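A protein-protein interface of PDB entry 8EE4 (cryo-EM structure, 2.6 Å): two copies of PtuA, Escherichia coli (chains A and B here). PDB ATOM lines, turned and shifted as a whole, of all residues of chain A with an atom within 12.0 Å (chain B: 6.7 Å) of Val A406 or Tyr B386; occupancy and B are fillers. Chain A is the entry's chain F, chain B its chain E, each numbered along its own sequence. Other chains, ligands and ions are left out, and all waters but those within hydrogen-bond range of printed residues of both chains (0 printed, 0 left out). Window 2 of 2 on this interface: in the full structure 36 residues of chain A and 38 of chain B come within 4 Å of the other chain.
The backbone carbonyl oxygen (O) of Gly B387 lies within hydrogen-bond range of the side-chain amide nitrogen (NE2) of Gln A403 (2.8 Å).
The side-chain carboxylate (OD1) of Asp A401 sits at hydrogen-bond distance from the backbone NH (N) of Gln A403 (2.7 Å). The backbone carbonyl oxygen (O) of Ser B358 is in hydrogen-bond range of the backbone NH (N) of Gly B387, at 3.1 Å.
Glu B388 touches Pro A402 (O to O, 3.98 Å). Glu B388 touches Gln A403 (N to NE2, 3.9 Å). CG of Pro A404 touches OG of Ser B358 (3.5 Å). Pro A404 touches Glu B388 (CD to O, 3.3 Å). Tyr B386 touches Val A406.
Printed residues of chain B within 4 Å of Pro A402: Glu B388 (3.98 Å). Printed residues of chain B within 4 Å of Gln A403: Gly B387 (2.8 Å) and Glu B388 (3.9 Å). Printed residues of chain B within 4 Å of Pro A404: Ser B358 (3.5 Å) and Glu B388 (3.3 Å). Val A406 touches one residue of chain B. Leu B357 touches none of the printed residues of chain A. Of the printed residues of chain A, Ser B358 touches Pro A404 (3.5 Å). No residue of chain A comes within 4 Å of Val B360. No residue of chain A comes within 4 Å of Ala B384. No residue of chain A comes within 4 Å of Thr B385. Of the printed residues of chain A, Tyr B386 touches Val A406. Gly B387 touches just one residue of chain A: Gln A403. Printed residues of chain A within 4 Å of Glu B388: Pro A402 (3.98 Å), Gln A403 (3.9 Å) and Pro A404 (3.3 Å). The nearest residue of chain A that does not touch Tyr B386 is Gln A403 (6.0 Å). The nearest printed residue of chain B that does not touch Pro A404 is Thr B359 (4.2 Å).
Of the 12 printed residues of chain B, 4 touch a printed residue of chain A. Of the 7 printed residues of chain A, 4 touch a printed residue of chain B. Among the printed residues, 6 pairs touch across the chains.
No position is printed for both chains. Of the 6 pairs that touch across the chains among the printed residues, none has its exchanged pair printed and touching as well.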
ATOM      1  N   VAL A 400     -17.957 -33.630 -14.586  1.00  0.00           N
ATOM      2  CA  VAL A 400     -18.466 -32.728 -13.559  1.00  0.00           C
ATOM      3  C   VAL A 400     -19.291 -33.553 -12.581  1.00  0.00           C
ATOM      4  O   VAL A 400     -20.299 -34.160 -12.965  1.00  0.00           O
ATOM      5  CB  VAL A 400     -19.301 -31.593 -14.171  1.00  0.00           C
ATOM      6  CG1 VAL A 400     -20.193 -30.949 -13.117  1.00  0.00           C
ATOM      7  CG2 VAL A 400     -18.393 -30.560 -14.817  1.00  0.00           C
ATOM      8  N   ASP A 401     -18.866 -33.573 -11.324  1.00  0.00           N
ATOM      9  CA  ASP A 401     -19.578 -34.343 -10.317  1.00  0.00           C
ATOM     10  C   ASP A 401     -20.972 -33.756 -10.105  1.00  0.00           C
ATOM     11  O   ASP A 401     -21.120 -32.533 -10.002  1.00  0.00           O
ATOM     12  CB  ASP A 401     -18.797 -34.345  -9.001  1.00  0.00           C
ATOM     13  CG  ASP A 401     -19.296 -35.393  -8.023  1.00  0.00           C
ATOM     14  OD1 ASP A 401     -20.522 -35.472  -7.802  1.00  0.00           O
ATOM     15  OD2 ASP A 401     -18.459 -36.137  -7.472  1.00  0.00           O
ATOM     16  N   PRO A 402     -22.018 -34.589 -10.033  1.00  0.00           N
ATOM     17  CA  PRO A 402     -23.358 -34.058  -9.745  1.00  0.00           C
ATOM     18  C   PRO A 402     -23.536 -33.577  -8.314  1.00  0.00           C
ATOM     19  O   PRO A 402     -24.594 -33.025  -7.994  1.00  0.00           O
ATOM     20  CB  PRO A 402     -24.277 -35.251 -10.043  1.00  0.00           C
ATOM     21  CG  PRO A 402     -23.420 -36.446  -9.851  1.00  0.00           C
ATOM     22  CD  PRO A 402     -22.043 -36.041 -10.284  1.00  0.00           C
ATOM     23  N   GLN A 403     -22.540 -33.765  -7.448  1.00  0.00           N
ATOM     24  CA  GLN A 403     -22.618 -33.314  -6.067  1.00  0.00           C
ATOM     25  C   GLN A 403     -21.983 -31.938  -5.955  1.00  0.00           C
ATOM     26  O   GLN A 403     -20.771 -31.814  -6.189  1.00  0.00           O
ATOM     27  CB  GLN A 403     -21.906 -34.301  -5.149  1.00  0.00           C
ATOM     28  CG  GLN A 403     -21.944 -33.942  -3.671  1.00  0.00           C
ATOM     29  CD  GLN A 403     -23.338 -34.022  -3.085  1.00  0.00           C
ATOM     30  OE1 GLN A 403     -23.932 -35.098  -3.009  1.00  0.00           O
ATOM     31  NE2 GLN A 403     -23.865 -32.883  -2.653  1.00  0.00           N
ATOM     32  N   PRO A 404     -22.730 -30.886  -5.613  1.00  0.00           N
ATOM     33  CA  PRO A 404     -22.099 -29.570  -5.457  1.00  0.00           C
ATOM     34  C   PRO A 404     -21.085 -29.572  -4.323  1.00  0.00           C
ATOM     35  O   PRO A 404     -21.251 -30.254  -3.310  1.00  0.00           O
ATOM     36  CB  PRO A 404     -23.278 -28.635  -5.154  1.00  0.00           C
ATOM     37  CG  PRO A 404     -24.504 -29.396  -5.523  1.00  0.00           C
ATOM     38  CD  PRO A 404     -24.176 -30.836  -5.346  1.00  0.00           C
ATOM     39  N   ALA A 405     -20.019 -28.792  -4.508  1.00  0.00           N
ATOM     40  CA  ALA A 405     -18.959 -28.671  -3.507  1.00  0.00           C
ATOM     41  C   ALA A 405     -19.325 -27.536  -2.554  1.00  0.00           C
ATOM     42  O   ALA A 405     -18.813 -26.418  -2.630  1.00  0.00           O
ATOM     43  CB  ALA A 405     -17.611 -28.438  -4.176  1.00  0.00           C
ATOM     44  N   VAL A 406     -20.236 -27.842  -1.636  1.00  0.00           N
ATOM     45  CA  VAL A 406     -20.709 -26.858  -0.670  1.00  0.00           C
ATOM     46  C   VAL A 406     -19.723 -26.745   0.485  1.00  0.00           C
ATOM     47  O   VAL A 406     -19.262 -27.750   1.024  1.00  0.00           O
ATOM     48  CB  VAL A 406     -22.118 -27.214  -0.151  1.00  0.00           C
ATOM     49  CG1 VAL A 406     -23.120 -27.218  -1.297  1.00  0.00           C
ATOM     50  CG2 VAL A 406     -22.109 -28.556   0.575  1.00  0.00           C
ATOM     51  N   LEU B 357     -30.194 -24.495  -8.319  1.00  0.00           N
ATOM     52  CA  LEU B 357     -31.130 -24.705  -7.221  1.00  0.00           C
ATOM     53  C   LEU B 357     -30.587 -25.628  -6.139  1.00  0.00           C
ATOM     54  O   LEU B 357     -31.171 -25.683  -5.052  1.00  0.00           O
ATOM     55  CB  LEU B 357     -32.445 -25.273  -7.761  1.00  0.00           C
ATOM     56  CG  LEU B 357     -33.336 -24.306  -8.546  1.00  0.00           C
ATOM     57  CD1 LEU B 357     -34.634 -24.985  -8.945  1.00  0.00           C
ATOM     58  CD2 LEU B 357     -33.622 -23.042  -7.751  1.00  0.00           C
ATOM     59  N   SER B 358     -29.501 -26.351  -6.399  1.00  0.00           N
ATOM     60  CA  SER B 358     -28.909 -27.232  -5.403  1.00  0.00           C
ATOM     61  C   SER B 358     -27.886 -26.525  -4.523  1.00  0.00           C
ATOM     62  O   SER B 358     -27.362 -27.145  -3.592  1.00  0.00           O
ATOM     63  CB  SER B 358     -28.250 -28.433  -6.087  1.00  0.00           C
ATOM     64  OG  SER B 358     -27.285 -28.014  -7.036  1.00  0.00           O
ATOM     65  N   THR B 359     -27.592 -25.255  -4.790  1.00  0.00           N
ATOM     66  CA  THR B 359     -26.599 -24.502  -4.039  1.00  0.00           C
ATOM     67  C   THR B 359     -27.220 -23.533  -3.040  1.00  0.00           C
ATOM     68  O   THR B 359     -26.492 -22.756  -2.416  1.00  0.00           O
ATOM     69  CB  THR B 359     -25.683 -23.742  -5.000  1.00  0.00           C
ATOM     70  OG1 THR B 359     -26.470 -23.092  -6.004  1.00  0.00           O
ATOM     71  CG2 THR B 359     -24.703 -24.698  -5.664  1.00  0.00           C
ATOM     72  N   VAL B 360     -28.544 -23.558  -2.873  1.00  0.00           N
ATOM     73  CA  VAL B 360     -29.225 -22.725  -1.893  1.00  0.00           C
ATOM     74  C   VAL B 360     -30.202 -23.595  -1.116  1.00  0.00           C
ATOM     75  O   VAL B 360     -30.648 -24.645  -1.582  1.00  0.00           O
ATOM     76  CB  VAL B 360     -29.968 -21.534  -2.538  1.00  0.00           C
ATOM     77  CG1 VAL B 360     -28.981 -20.561  -3.156  1.00  0.00           C
ATOM     78  CG2 VAL B 360     -30.970 -22.019  -3.572  1.00  0.00           C
ATOM     79  N   LYS B 361     -30.532 -23.139   0.088  1.00  0.00           N
ATOM     80  CA  LYS B 361     -31.474 -23.853   0.932  1.00  0.00           C
ATOM     81  C   LYS B 361     -32.904 -23.588   0.470  1.00  0.00           C
ATOM     82  O   LYS B 361     -33.180 -22.645  -0.275  1.00  0.00           O
ATOM     83  CB  LYS B 361     -31.293 -23.443   2.393  1.00  0.00           C
ATOM     84  CG  LYS B 361     -29.989 -23.938   2.997  1.00  0.00           C
ATOM     85  CD  LYS B 361     -29.481 -23.015   4.091  1.00  0.00           C
ATOM     86  CE  LYS B 361     -28.158 -23.508   4.657  1.00  0.00           C
ATOM     87  NZ  LYS B 361     -28.312 -24.751   5.460  1.00  0.00           N
ATOM     88  N   ARG B 362     -33.823 -24.440   0.925  1.00  0.00           N
ATOM     89  CA  ARG B 362     -35.207 -24.343   0.480  1.00  0.00           C
ATOM     90  C   ARG B 362     -35.888 -23.066   0.955  1.00  0.00           C
ATOM     91  O   ARG B 362     -36.973 -22.745   0.460  1.00  0.00           O
ATOM     92  CB  ARG B 362     -35.998 -25.563   0.956  1.00  0.00           C
ATOM     93  CG  ARG B 362     -36.431 -25.519   2.413  1.00  0.00           C
ATOM     94  CD  ARG B 362     -37.129 -26.809   2.814  1.00  0.00           C
ATOM     95  NE  ARG B 362     -38.576 -26.724   2.655  1.00  0.00           N
ATOM     96  CZ  ARG B 362     -39.418 -26.306   3.591  1.00  0.00           C
ATOM     97  NH1 ARG B 362     -38.993 -25.917   4.783  1.00  0.00           N
ATOM     98  NH2 ARG B 362     -40.720 -26.275   3.325  1.00  0.00           N
ATOM     99  N   ALA B 384     -35.683 -31.227   0.484  1.00  0.00           N
ATOM    100  CA  ALA B 384     -34.432 -30.504   0.651  1.00  0.00           C
ATOM    101  C   ALA B 384     -33.736 -30.322  -0.692  1.00  0.00           C
ATOM    102  O   ALA B 384     -33.915 -31.114  -1.620  1.00  0.00           O
ATOM    103  CB  ALA B 384     -33.506 -31.243   1.620  1.00  0.00           C
ATOM    104  N   THR B 385     -32.939 -29.257  -0.785  1.00  0.00           N
ATOM    105  CA  THR B 385     -32.177 -28.961  -1.988  1.00  0.00           C
ATOM    106  C   THR B 385     -30.728 -28.591  -1.716  1.00  0.00           C
ATOM    107  O   THR B 385     -29.936 -28.554  -2.663  1.00  0.00           O
ATOM    108  CB  THR B 385     -32.832 -27.814  -2.775  1.00  0.00           C
ATOM    109  OG1 THR B 385     -33.109 -26.720  -1.891  1.00  0.00           O
ATOM    110  CG2 THR B 385     -34.127 -28.276  -3.426  1.00  0.00           C
ATOM    111  N   TYR B 386     -30.355 -28.323  -0.468  1.00  0.00           N
ATOM    112  CA  TYR B 386     -29.002 -27.881  -0.159  1.00  0.00           C
ATOM    113  C   TYR B 386     -28.036 -29.059  -0.242  1.00  0.00           C
ATOM    114  O   TYR B 386     -28.179 -30.041   0.494  1.00  0.00           O
ATOM    115  CB  TYR B 386     -28.965 -27.252   1.230  1.00  0.00           C
ATOM    116  CG  TYR B 386     -27.622 -26.668   1.607  1.00  0.00           C
ATOM    117  CD1 TYR B 386     -27.151 -25.514   0.998  1.00  0.00           C
ATOM    118  CD2 TYR B 386     -26.827 -27.270   2.573  1.00  0.00           C
ATOM    119  CE1 TYR B 386     -25.927 -24.975   1.339  1.00  0.00           C
ATOM    120  CE2 TYR B 386     -25.600 -26.739   2.921  1.00  0.00           C
ATOM    121  CZ  TYR B 386     -25.155 -25.591   2.300  1.00  0.00           C
ATOM    122  OH  TYR B 386     -23.934 -25.059   2.643  1.00  0.00           O
ATOM    123  N   GLY B 387     -27.056 -28.957  -1.134  1.00  0.00           N
ATOM    124  CA  GLY B 387     -26.044 -29.996  -1.250  1.00  0.00           C
ATOM    125  C   GLY B 387     -26.587 -31.338  -1.687  1.00  0.00           C
ATOM    126  O   GLY B 387     -26.208 -32.371  -1.120  1.00  0.00           O
ATOM    127  N   GLU B 388     -27.471 -31.350  -2.683  1.00  0.00           N
ATOM    128  CA  GLU B 388     -28.053 -32.579  -3.193  1.00  0.00           C
ATOM    129  C   GLU B 388     -27.638 -32.801  -4.644  1.00  0.00           C
ATOM    130  O   GLU B 388     -27.340 -31.840  -5.361  1.00  0.00           O
ATOM    131  CB  GLU B 388     -29.584 -32.546  -3.108  1.00  0.00           C
ATOM    132  CG  GLU B 388     -30.136 -32.846  -1.725  1.00  0.00           C
ATOM    133  CD  GLU B 388     -31.639 -33.047  -1.730  1.00  0.00           C
ATOM    134  OE1 GLU B 388     -32.247 -32.979  -2.818  1.00  0.00           O
ATOM    135  OE2 GLU B 388     -32.213 -33.275  -0.645  1.00  0.00           O
ATOM    136  N   VAL B 393     -32.997 -32.756  -7.145  1.00  0.00           N
ATOM    137  CA  VAL B 393     -33.701 -31.486  -7.295  1.00  0.00           C
ATOM    138  C   VAL B 393     -34.559 -31.507  -8.552  1.00  0.00           C
ATOM    139  O   VAL B 393     -35.690 -31.006  -8.558  1.00  0.00           O
ATOM    140  CB  VAL B 393     -32.698 -30.319  -7.318  1.00  0.00           C
ATOM    141  CG1 VAL B 393     -33.428 -28.995  -7.480  1.00  0.00           C
ATOM    142  CG2 VAL B 393     -31.850 -30.318  -6.057  1.00  0.00           C
